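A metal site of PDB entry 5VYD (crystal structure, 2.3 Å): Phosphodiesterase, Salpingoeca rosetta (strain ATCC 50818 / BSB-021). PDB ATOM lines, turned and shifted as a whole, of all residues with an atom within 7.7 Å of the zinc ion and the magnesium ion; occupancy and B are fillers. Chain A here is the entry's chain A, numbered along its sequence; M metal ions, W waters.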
ATOM      1  N   TYR A  60     -14.551  11.908  -3.281  1.00  0.00           N
ATOM      2  CA  TYR A  60     -14.381  11.314  -4.604  1.00  0.00           C
ATOM      3  C   TYR A  60     -15.383  11.925  -5.574  1.00  0.00           C
ATOM      4  O   TYR A  60     -16.483  12.336  -5.206  1.00  0.00           O
ATOM      5  CB  TYR A  60     -14.560   9.791  -4.543  1.00  0.00           C
ATOM      6  CG  TYR A  60     -13.307   9.058  -4.117  1.00  0.00           C
ATOM      7  CD1 TYR A  60     -12.986   8.914  -2.774  1.00  0.00           C
ATOM      8  CD2 TYR A  60     -12.446   8.517  -5.057  1.00  0.00           C
ATOM      9  CE1 TYR A  60     -11.833   8.249  -2.385  1.00  0.00           C
ATOM     10  CE2 TYR A  60     -11.293   7.860  -4.683  1.00  0.00           C
ATOM     11  CZ  TYR A  60     -11.000   7.729  -3.340  1.00  0.00           C
ATOM     12  OH  TYR A  60      -9.847   7.064  -2.951  1.00  0.00           O
ATOM     13  N   PHE A  65     -14.093   5.328 -13.740  1.00  0.00           N
ATOM     14  CA  PHE A  65     -13.200   4.409 -13.031  1.00  0.00           C
ATOM     15  C   PHE A  65     -12.792   4.946 -11.661  1.00  0.00           C
ATOM     16  O   PHE A  65     -13.078   4.319 -10.637  1.00  0.00           O
ATOM     17  CB  PHE A  65     -11.952   4.102 -13.876  1.00  0.00           C
ATOM     18  CG  PHE A  65     -11.065   3.033 -13.280  1.00  0.00           C
ATOM     19  CD1 PHE A  65     -10.106   3.353 -12.322  1.00  0.00           C
ATOM     20  CD2 PHE A  65     -11.194   1.716 -13.671  1.00  0.00           C
ATOM     21  CE1 PHE A  65      -9.294   2.369 -11.774  1.00  0.00           C
ATOM     22  CE2 PHE A  65     -10.387   0.728 -13.131  1.00  0.00           C
ATOM     23  CZ  PHE A  65      -9.436   1.055 -12.182  1.00  0.00           C
ATOM     24  N   HIS A  66     -12.109   6.092 -11.614  1.00  0.00           N
ATOM     25  CA  HIS A  66     -11.527   6.605 -10.372  1.00  0.00           C
ATOM     26  C   HIS A  66     -12.606   7.246  -9.506  1.00  0.00           C
ATOM     27  O   HIS A  66     -12.681   8.461  -9.319  1.00  0.00           O
ATOM     28  CB  HIS A  66     -10.388   7.573 -10.666  1.00  0.00           C
ATOM     29  CG  HIS A  66      -9.183   6.918 -11.258  1.00  0.00           C
ATOM     30  ND1 HIS A  66      -8.946   6.858 -12.620  1.00  0.00           N
ATOM     31  CD2 HIS A  66      -8.144   6.275 -10.677  1.00  0.00           C
ATOM     32  CE1 HIS A  66      -7.812   6.209 -12.841  1.00  0.00           C
ATOM     33  NE2 HIS A  66      -7.310   5.842 -11.679  1.00  0.00           N
ATOM     34  N   ASN A  67     -13.454   6.386  -8.954  1.00  0.00           N
ATOM     35  CA  ASN A  67     -14.598   6.774  -8.134  1.00  0.00           C
ATOM     36  C   ASN A  67     -14.499   6.096  -6.776  1.00  0.00           C
ATOM     37  O   ASN A  67     -13.549   5.361  -6.479  1.00  0.00           O
ATOM     38  CB  ASN A  67     -15.917   6.434  -8.837  1.00  0.00           C
ATOM     39  CG  ASN A  67     -15.951   5.006  -9.347  1.00  0.00           C
ATOM     40  OD1 ASN A  67     -15.617   4.077  -8.622  1.00  0.00           O
ATOM     41  ND2 ASN A  67     -16.352   4.834 -10.602  1.00  0.00           N
ATOM     42  N   HIS A  70     -14.045   2.344  -6.817  1.00  0.00           N
ATOM     43  CA  HIS A  70     -12.668   1.917  -6.995  1.00  0.00           C
ATOM     44  C   HIS A  70     -11.914   1.926  -5.668  1.00  0.00           C
ATOM     45  O   HIS A  70     -11.122   1.021  -5.389  1.00  0.00           O
ATOM     46  CB  HIS A  70     -11.964   2.824  -8.011  1.00  0.00           C
ATOM     47  CG  HIS A  70     -10.485   2.620  -8.079  1.00  0.00           C
ATOM     48  ND1 HIS A  70      -9.912   1.397  -8.337  1.00  0.00           N
ATOM     49  CD2 HIS A  70      -9.453   3.490  -7.925  1.00  0.00           C
ATOM     50  CE1 HIS A  70      -8.592   1.518  -8.340  1.00  0.00           C
ATOM     51  NE2 HIS A  70      -8.291   2.776  -8.088  1.00  0.00           N
ATOM     52  N   ALA A  71     -12.163   2.944  -4.837  1.00  0.00           N
ATOM     53  CA  ALA A  71     -11.466   3.032  -3.554  1.00  0.00           C
ATOM     54  C   ALA A  71     -11.871   1.891  -2.627  1.00  0.00           C
ATOM     55  O   ALA A  71     -11.043   1.350  -1.899  1.00  0.00           O
ATOM     56  CB  ALA A  71     -11.746   4.380  -2.895  1.00  0.00           C
ATOM     57  N   VAL A  74     -10.126  -1.185  -3.789  1.00  0.00           N
ATOM     58  CA  VAL A  74      -8.738  -1.226  -3.358  1.00  0.00           C
ATOM     59  C   VAL A  74      -8.643  -1.595  -1.880  1.00  0.00           C
ATOM     60  O   VAL A  74      -7.810  -2.411  -1.487  1.00  0.00           O
ATOM     61  CB  VAL A  74      -8.052   0.121  -3.656  1.00  0.00           C
ATOM     62  CG1 VAL A  74      -6.703   0.216  -2.952  1.00  0.00           C
ATOM     63  CG2 VAL A  74      -7.866   0.275  -5.158  1.00  0.00           C
ATOM     64  N   ALA A 102      -5.652   2.949   1.409  1.00  0.00           N
ATOM     65  CA  ALA A 102      -6.401   2.348   0.312  1.00  0.00           C
ATOM     66  C   ALA A 102      -7.652   3.155  -0.006  1.00  0.00           C
ATOM     67  O   ALA A 102      -7.966   3.398  -1.179  1.00  0.00           O
ATOM     68  CB  ALA A 102      -6.758   0.907   0.646  1.00  0.00           C
ATOM     69  N   HIS A 105      -6.524   6.783  -1.564  1.00  0.00           N
ATOM     70  CA  HIS A 105      -5.394   6.839  -2.487  1.00  0.00           C
ATOM     71  C   HIS A 105      -5.704   7.523  -3.809  1.00  0.00           C
ATOM     72  O   HIS A 105      -4.770   7.827  -4.564  1.00  0.00           O
ATOM     73  CB  HIS A 105      -4.872   5.424  -2.774  1.00  0.00           C
ATOM     74  CG  HIS A 105      -5.639   4.699  -3.824  1.00  0.00           C
ATOM     75  ND1 HIS A 105      -6.864   4.120  -3.589  1.00  0.00           N
ATOM     76  CD2 HIS A 105      -5.361   4.471  -5.134  1.00  0.00           C
ATOM     77  CE1 HIS A 105      -7.317   3.566  -4.697  1.00  0.00           C
ATOM     78  NE2 HIS A 105      -6.418   3.758  -5.649  1.00  0.00           N
ATOM     79  N   ASP A 106      -6.983   7.768  -4.128  1.00  0.00           N
ATOM     80  CA  ASP A 106      -7.354   8.450  -5.361  1.00  0.00           C
ATOM     81  C   ASP A 106      -8.326   9.595  -5.089  1.00  0.00           C
ATOM     82  O   ASP A 106      -9.192   9.901  -5.926  1.00  0.00           O
ATOM     83  CB  ASP A 106      -7.976   7.479  -6.371  1.00  0.00           C
ATOM     84  CG  ASP A 106      -6.936   6.804  -7.248  1.00  0.00           C
ATOM     85  OD1 ASP A 106      -5.835   7.357  -7.418  1.00  0.00           O
ATOM     86  OD2 ASP A 106      -7.234   5.716  -7.783  1.00  0.00           O
ATOM     87  N   LEU A 107      -8.212  10.235  -3.931  1.00  0.00           N
ATOM     88  CA  LEU A 107      -9.129  11.308  -3.566  1.00  0.00           C
ATOM     89  C   LEU A 107      -9.086  12.447  -4.582  1.00  0.00           C
ATOM     90  O   LEU A 107      -8.013  12.878  -5.011  1.00  0.00           O
ATOM     91  CB  LEU A 107      -8.801  11.847  -2.169  1.00  0.00           C
ATOM     92  CG  LEU A 107      -9.339  11.056  -0.980  1.00  0.00           C
ATOM     93  CD1 LEU A 107      -8.671  11.540   0.305  1.00  0.00           C
ATOM     94  CD2 LEU A 107     -10.844  11.206  -0.874  1.00  0.00           C
ATOM     95  N   HIS A 109      -9.728  12.516  -7.634  1.00  0.00           N
ATOM     96  CA  HIS A 109      -9.364  12.175  -9.007  1.00  0.00           C
ATOM     97  C   HIS A 109     -10.432  12.671  -9.976  1.00  0.00           C
ATOM     98  O   HIS A 109     -11.629  12.623  -9.679  1.00  0.00           O
ATOM     99  CB  HIS A 109      -9.175  10.658  -9.125  1.00  0.00           C
ATOM    100  CG  HIS A 109      -8.255  10.243 -10.228  1.00  0.00           C
ATOM    101  ND1 HIS A 109      -8.645  10.208 -11.556  1.00  0.00           N
ATOM    102  CD2 HIS A 109      -6.971   9.814 -10.206  1.00  0.00           C
ATOM    103  CE1 HIS A 109      -7.633   9.786 -12.290  1.00  0.00           C
ATOM    104  NE2 HIS A 109      -6.609   9.530 -11.499  1.00  0.00           N
ATOM    105  N   ASN A 114      -1.492  12.093 -14.788  1.00  0.00           N
ATOM    106  CA  ASN A 114      -0.411  13.030 -14.478  1.00  0.00           C
ATOM    107  C   ASN A 114       0.090  13.734 -15.723  1.00  0.00           C
ATOM    108  O   ASN A 114       0.411  14.927 -15.684  1.00  0.00           O
ATOM    109  CB  ASN A 114       0.742  12.293 -13.797  1.00  0.00           C
ATOM    110  CG  ASN A 114       0.493  12.063 -12.313  1.00  0.00           C
ATOM    111  OD1 ASN A 114      -0.340  12.730 -11.704  1.00  0.00           O
ATOM    112  ND2 ASN A 114       1.222  11.111 -11.736  1.00  0.00           N
ATOM    113  N   LEU A 134      -0.850  13.817  -9.197  1.00  0.00           N
ATOM    114  CA  LEU A 134      -2.081  13.263  -8.654  1.00  0.00           C
ATOM    115  C   LEU A 134      -1.867  12.679  -7.270  1.00  0.00           C
ATOM    116  O   LEU A 134      -2.608  12.980  -6.327  1.00  0.00           O
ATOM    117  CB  LEU A 134      -2.634  12.189  -9.593  1.00  0.00           C
ATOM    118  CG  LEU A 134      -3.806  12.522 -10.519  1.00  0.00           C
ATOM    119  CD1 LEU A 134      -3.951  14.016 -10.709  1.00  0.00           C
ATOM    120  CD2 LEU A 134      -3.579  11.829 -11.840  1.00  0.00           C
ATOM    121  N   GLU A 135      -0.856  11.817  -7.126  1.00  0.00           N
ATOM    122  CA  GLU A 135      -0.668  11.069  -5.886  1.00  0.00           C
ATOM    123  C   GLU A 135      -0.343  11.997  -4.728  1.00  0.00           C
ATOM    124  O   GLU A 135      -0.818  11.787  -3.607  1.00  0.00           O
ATOM    125  CB  GLU A 135       0.410  10.015  -6.074  1.00  0.00           C
ATOM    126  CG  GLU A 135       0.019   8.864  -7.014  1.00  0.00           C
ATOM    127  CD  GLU A 135      -0.120   9.287  -8.471  1.00  0.00           C
ATOM    128  OE1 GLU A 135       0.386  10.374  -8.839  1.00  0.00           O
ATOM    129  OE2 GLU A 135      -0.748   8.537  -9.263  1.00  0.00           O
ATOM    130  N   HIS A 138      -3.668  13.409  -3.755  1.00  0.00           N
ATOM    131  CA  HIS A 138      -4.475  12.442  -3.000  1.00  0.00           C
ATOM    132  C   HIS A 138      -4.008  12.351  -1.559  1.00  0.00           C
ATOM    133  O   HIS A 138      -4.812  12.397  -0.626  1.00  0.00           O
ATOM    134  CB  HIS A 138      -4.408  11.058  -3.669  1.00  0.00           C
ATOM    135  CG  HIS A 138      -4.798  11.056  -5.110  1.00  0.00           C
ATOM    136  ND1 HIS A 138      -5.811  11.836  -5.623  1.00  0.00           N
ATOM    137  CD2 HIS A 138      -4.309  10.348  -6.156  1.00  0.00           C
ATOM    138  CE1 HIS A 138      -5.929  11.606  -6.914  1.00  0.00           C
ATOM    139  NE2 HIS A 138      -5.023  10.713  -7.267  1.00  0.00           N
ATOM    140  N   ILE A 173       0.604   5.661  -0.883  1.00  0.00           N
ATOM    141  CA  ILE A 173      -0.156   6.417  -1.879  1.00  0.00           C
ATOM    142  C   ILE A 173       0.767   6.906  -2.987  1.00  0.00           C
ATOM    143  O   ILE A 173       0.441   6.791  -4.175  1.00  0.00           O
ATOM    144  CB  ILE A 173      -0.904   7.580  -1.206  1.00  0.00           C
ATOM    145  CG1 ILE A 173      -1.968   7.042  -0.238  1.00  0.00           C
ATOM    146  CG2 ILE A 173      -1.544   8.479  -2.261  1.00  0.00           C
ATOM    147  CD1 ILE A 173      -2.876   8.103   0.327  1.00  0.00           C
ATOM    148  N   THR A 176       1.527   4.415  -5.671  1.00  0.00           N
ATOM    149  CA  THR A 176       0.534   4.014  -6.663  1.00  0.00           C
ATOM    150  C   THR A 176       0.744   4.707  -8.003  1.00  0.00           C
ATOM    151  O   THR A 176       0.067   4.365  -8.973  1.00  0.00           O
ATOM    152  CB  THR A 176      -0.887   4.286  -6.170  1.00  0.00           C
ATOM    153  OG1 THR A 176      -1.066   5.684  -5.911  1.00  0.00           O
ATOM    154  CG2 THR A 176      -1.193   3.486  -4.902  1.00  0.00           C
ATOM    155  N   ASP A 177       1.671   5.660  -8.077  1.00  0.00           N
ATOM    156  CA  ASP A 177       2.022   6.283  -9.342  1.00  0.00           C
ATOM    157  C   ASP A 177       2.707   5.259 -10.242  1.00  0.00           C
ATOM    158  O   ASP A 177       3.717   4.658  -9.847  1.00  0.00           O
ATOM    159  CB  ASP A 177       2.926   7.490  -9.111  1.00  0.00           C
ATOM    160  CG  ASP A 177       3.230   8.255 -10.390  1.00  0.00           C
ATOM    161  OD1 ASP A 177       2.570   8.003 -11.419  1.00  0.00           O
ATOM    162  OD2 ASP A 177       4.140   9.104 -10.374  1.00  0.00           O
ATOM    163  N   MET A 178       2.165   5.054 -11.441  1.00  0.00           N
ATOM    164  CA  MET A 178       2.727   4.065 -12.349  1.00  0.00           C
ATOM    165  C   MET A 178       4.163   4.391 -12.748  1.00  0.00           C
ATOM    166  O   MET A 178       4.895   3.485 -13.158  1.00  0.00           O
ATOM    167  CB  MET A 178       1.857   3.939 -13.605  1.00  0.00           C
ATOM    168  CG  MET A 178       0.600   3.097 -13.410  1.00  0.00           C
ATOM    169  SD  MET A 178       0.967   1.402 -12.908  1.00  0.00           S
ATOM    170  CE  MET A 178       2.108   0.892 -14.193  1.00  0.00           C
ATOM    171  N   LEU A 215      -0.214  -2.347  -1.653  1.00  0.00           N
ATOM    172  CA  LEU A 215      -1.226  -1.363  -2.045  1.00  0.00           C
ATOM    173  C   LEU A 215      -1.238  -1.177  -3.556  1.00  0.00           C
ATOM    174  O   LEU A 215      -2.304  -1.103  -4.172  1.00  0.00           O
ATOM    175  CB  LEU A 215      -0.995  -0.029  -1.337  1.00  0.00           C
ATOM    176  CG  LEU A 215      -2.131   0.944  -1.645  1.00  0.00           C
ATOM    177  CD1 LEU A 215      -3.437   0.388  -1.103  1.00  0.00           C
ATOM    178  CD2 LEU A 215      -1.855   2.336  -1.102  1.00  0.00           C
ATOM    179  N   ALA A 218      -3.064  -4.053  -5.018  1.00  0.00           N
ATOM    180  CA  ALA A 218      -4.502  -3.933  -4.844  1.00  0.00           C
ATOM    181  C   ALA A 218      -5.086  -2.864  -5.763  1.00  0.00           C
ATOM    182  O   ALA A 218      -6.242  -2.994  -6.189  1.00  0.00           O
ATOM    183  CB  ALA A 218      -4.837  -3.609  -3.383  1.00  0.00           C
ATOM    184  N   ASP A 219      -4.323  -1.826  -6.078  1.00  0.00           N
ATOM    185  CA  ASP A 219      -4.783  -0.805  -7.009  1.00  0.00           C
ATOM    186  C   ASP A 219      -5.067  -1.391  -8.390  1.00  0.00           C
ATOM    187  O   ASP A 219      -6.018  -0.984  -9.061  1.00  0.00           O
ATOM    188  CB  ASP A 219      -3.753   0.325  -7.106  1.00  0.00           C
ATOM    189  CG  ASP A 219      -4.324   1.593  -7.734  1.00  0.00           C
ATOM    190  OD1 ASP A 219      -5.555   1.752  -7.748  1.00  0.00           O
ATOM    191  OD2 ASP A 219      -3.519   2.432  -8.212  1.00  0.00           O
ATOM    192  N   LEU A 220      -4.264  -2.371  -8.805  1.00  0.00           N
ATOM    193  CA  LEU A 220      -4.414  -3.008 -10.117  1.00  0.00           C
ATOM    194  C   LEU A 220      -5.301  -4.251 -10.005  1.00  0.00           C
ATOM    195  O   LEU A 220      -4.918  -5.360 -10.359  1.00  0.00           O
ATOM    196  CB  LEU A 220      -3.043  -3.362 -10.683  1.00  0.00           C
ATOM    197  CG  LEU A 220      -2.174  -2.327 -11.405  1.00  0.00           C
ATOM    198  CD1 LEU A 220      -2.177  -0.963 -10.720  1.00  0.00           C
ATOM    199  CD2 LEU A 220      -0.747  -2.851 -11.501  1.00  0.00           C
ATOM    200  N   HIS A 221      -6.518  -4.023  -9.514  1.00  0.00           N
ATOM    201  CA  HIS A 221      -7.424  -5.128  -9.206  1.00  0.00           C
ATOM    202  C   HIS A 221      -8.187  -5.658 -10.410  1.00  0.00           C
ATOM    203  O   HIS A 221      -8.894  -6.662 -10.284  1.00  0.00           O
ATOM    204  CB  HIS A 221      -8.419  -4.707  -8.119  1.00  0.00           C
ATOM    205  CG  HIS A 221      -9.236  -3.508  -8.484  1.00  0.00           C
ATOM    206  ND1 HIS A 221     -10.283  -3.556  -9.379  1.00  0.00           N
ATOM    207  CD2 HIS A 221      -9.154  -2.221  -8.063  1.00  0.00           C
ATOM    208  CE1 HIS A 221     -10.811  -2.348  -9.496  1.00  0.00           C
ATOM    209  NE2 HIS A 221     -10.148  -1.524  -8.706  1.00  0.00           N
HETATM  210 ZN    ZN M   1      -6.331   3.790  -7.854  1.00  0.00          ZN
HETATM  211 MG    MG M   2      -4.161   6.703  -8.654  1.00  0.00          MG
HETATM  212  O   HOH W   1      -4.972   6.322 -10.615  1.00  0.00           O
HETATM  213  O   HOH W   2      -6.044   3.947 -10.391  1.00  0.00           O
HETATM  214  O   HOH W   3      -2.016   6.410  -9.096  1.00  0.00           O
HETATM  215  O   HOH W   4      -3.191   7.077  -6.594  1.00  0.00           O
HETATM  216  O   HOH W   5      -4.514   4.791  -8.339  1.00  0.00           O
HETATM  217  O   HOH W   6      -3.794   8.761  -9.225  1.00  0.00           O
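OD1 of Asp 106 sits close to NE2 of His 138 (3.5 Å).
The side-chain hydroxyl of Tyr 60 is in hydrogen-bond range of the backbone NH of Asp 106 (3.2 Å).
A ring nitrogen (ND1) of His 105 lies within hydrogen-bond range of the backbone carbonyl oxygen (O) of Ala 102, 2.7 Å away.
A ring nitrogen (ND1) of His 70 sits at hydrogen-bond distance from a ring nitrogen (NE2) of His 221.
OD1 of Asn 67 lies within hydrogen-bond range of N of His 70, 3.0 Å away.
The side-chain carboxylate of Glu 135 sits at hydrogen-bond distance from the side-chain amide nitrogen of Asn 114, at 3.1 Å.
Four residues have an atom within 4 Å of the zinc ion: His 70, His 105, Asp 106 and Asp 219.
The nearest printed residue that does not touch the zinc ion is His 66 (4.2 Å).
The magnesium ion is bound by water W5 (2.0 Å), water W1 (2.2 Å), water W6 (2.2 Å), OD1 of Asp 106 (2.2 Å), water W3 (2.2 Å) and water W4 (2.3 Å).
Merely in contact with the magnesium ion: Glu 135 (3.9 Å).
The zinc ion is bound by OD2 of Asp 106, water W5, OD1 of Asp 219, NE2 of His 105, NE2 of His 70 and water W2.
The zinc ion has six donor atoms within binding distance.
Water W6 bridges a ring nitrogen (NE2) of His 138 (3.0 Å) and the side-chain carboxylate (OE2) of Glu 135 (3.1 Å).
Water W3 bridges OE2 of Glu 135 and O of Thr 176.
Water W4 bridges OG1 of Thr 176 (2.6 Å) and O of His 105 (2.7 Å).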
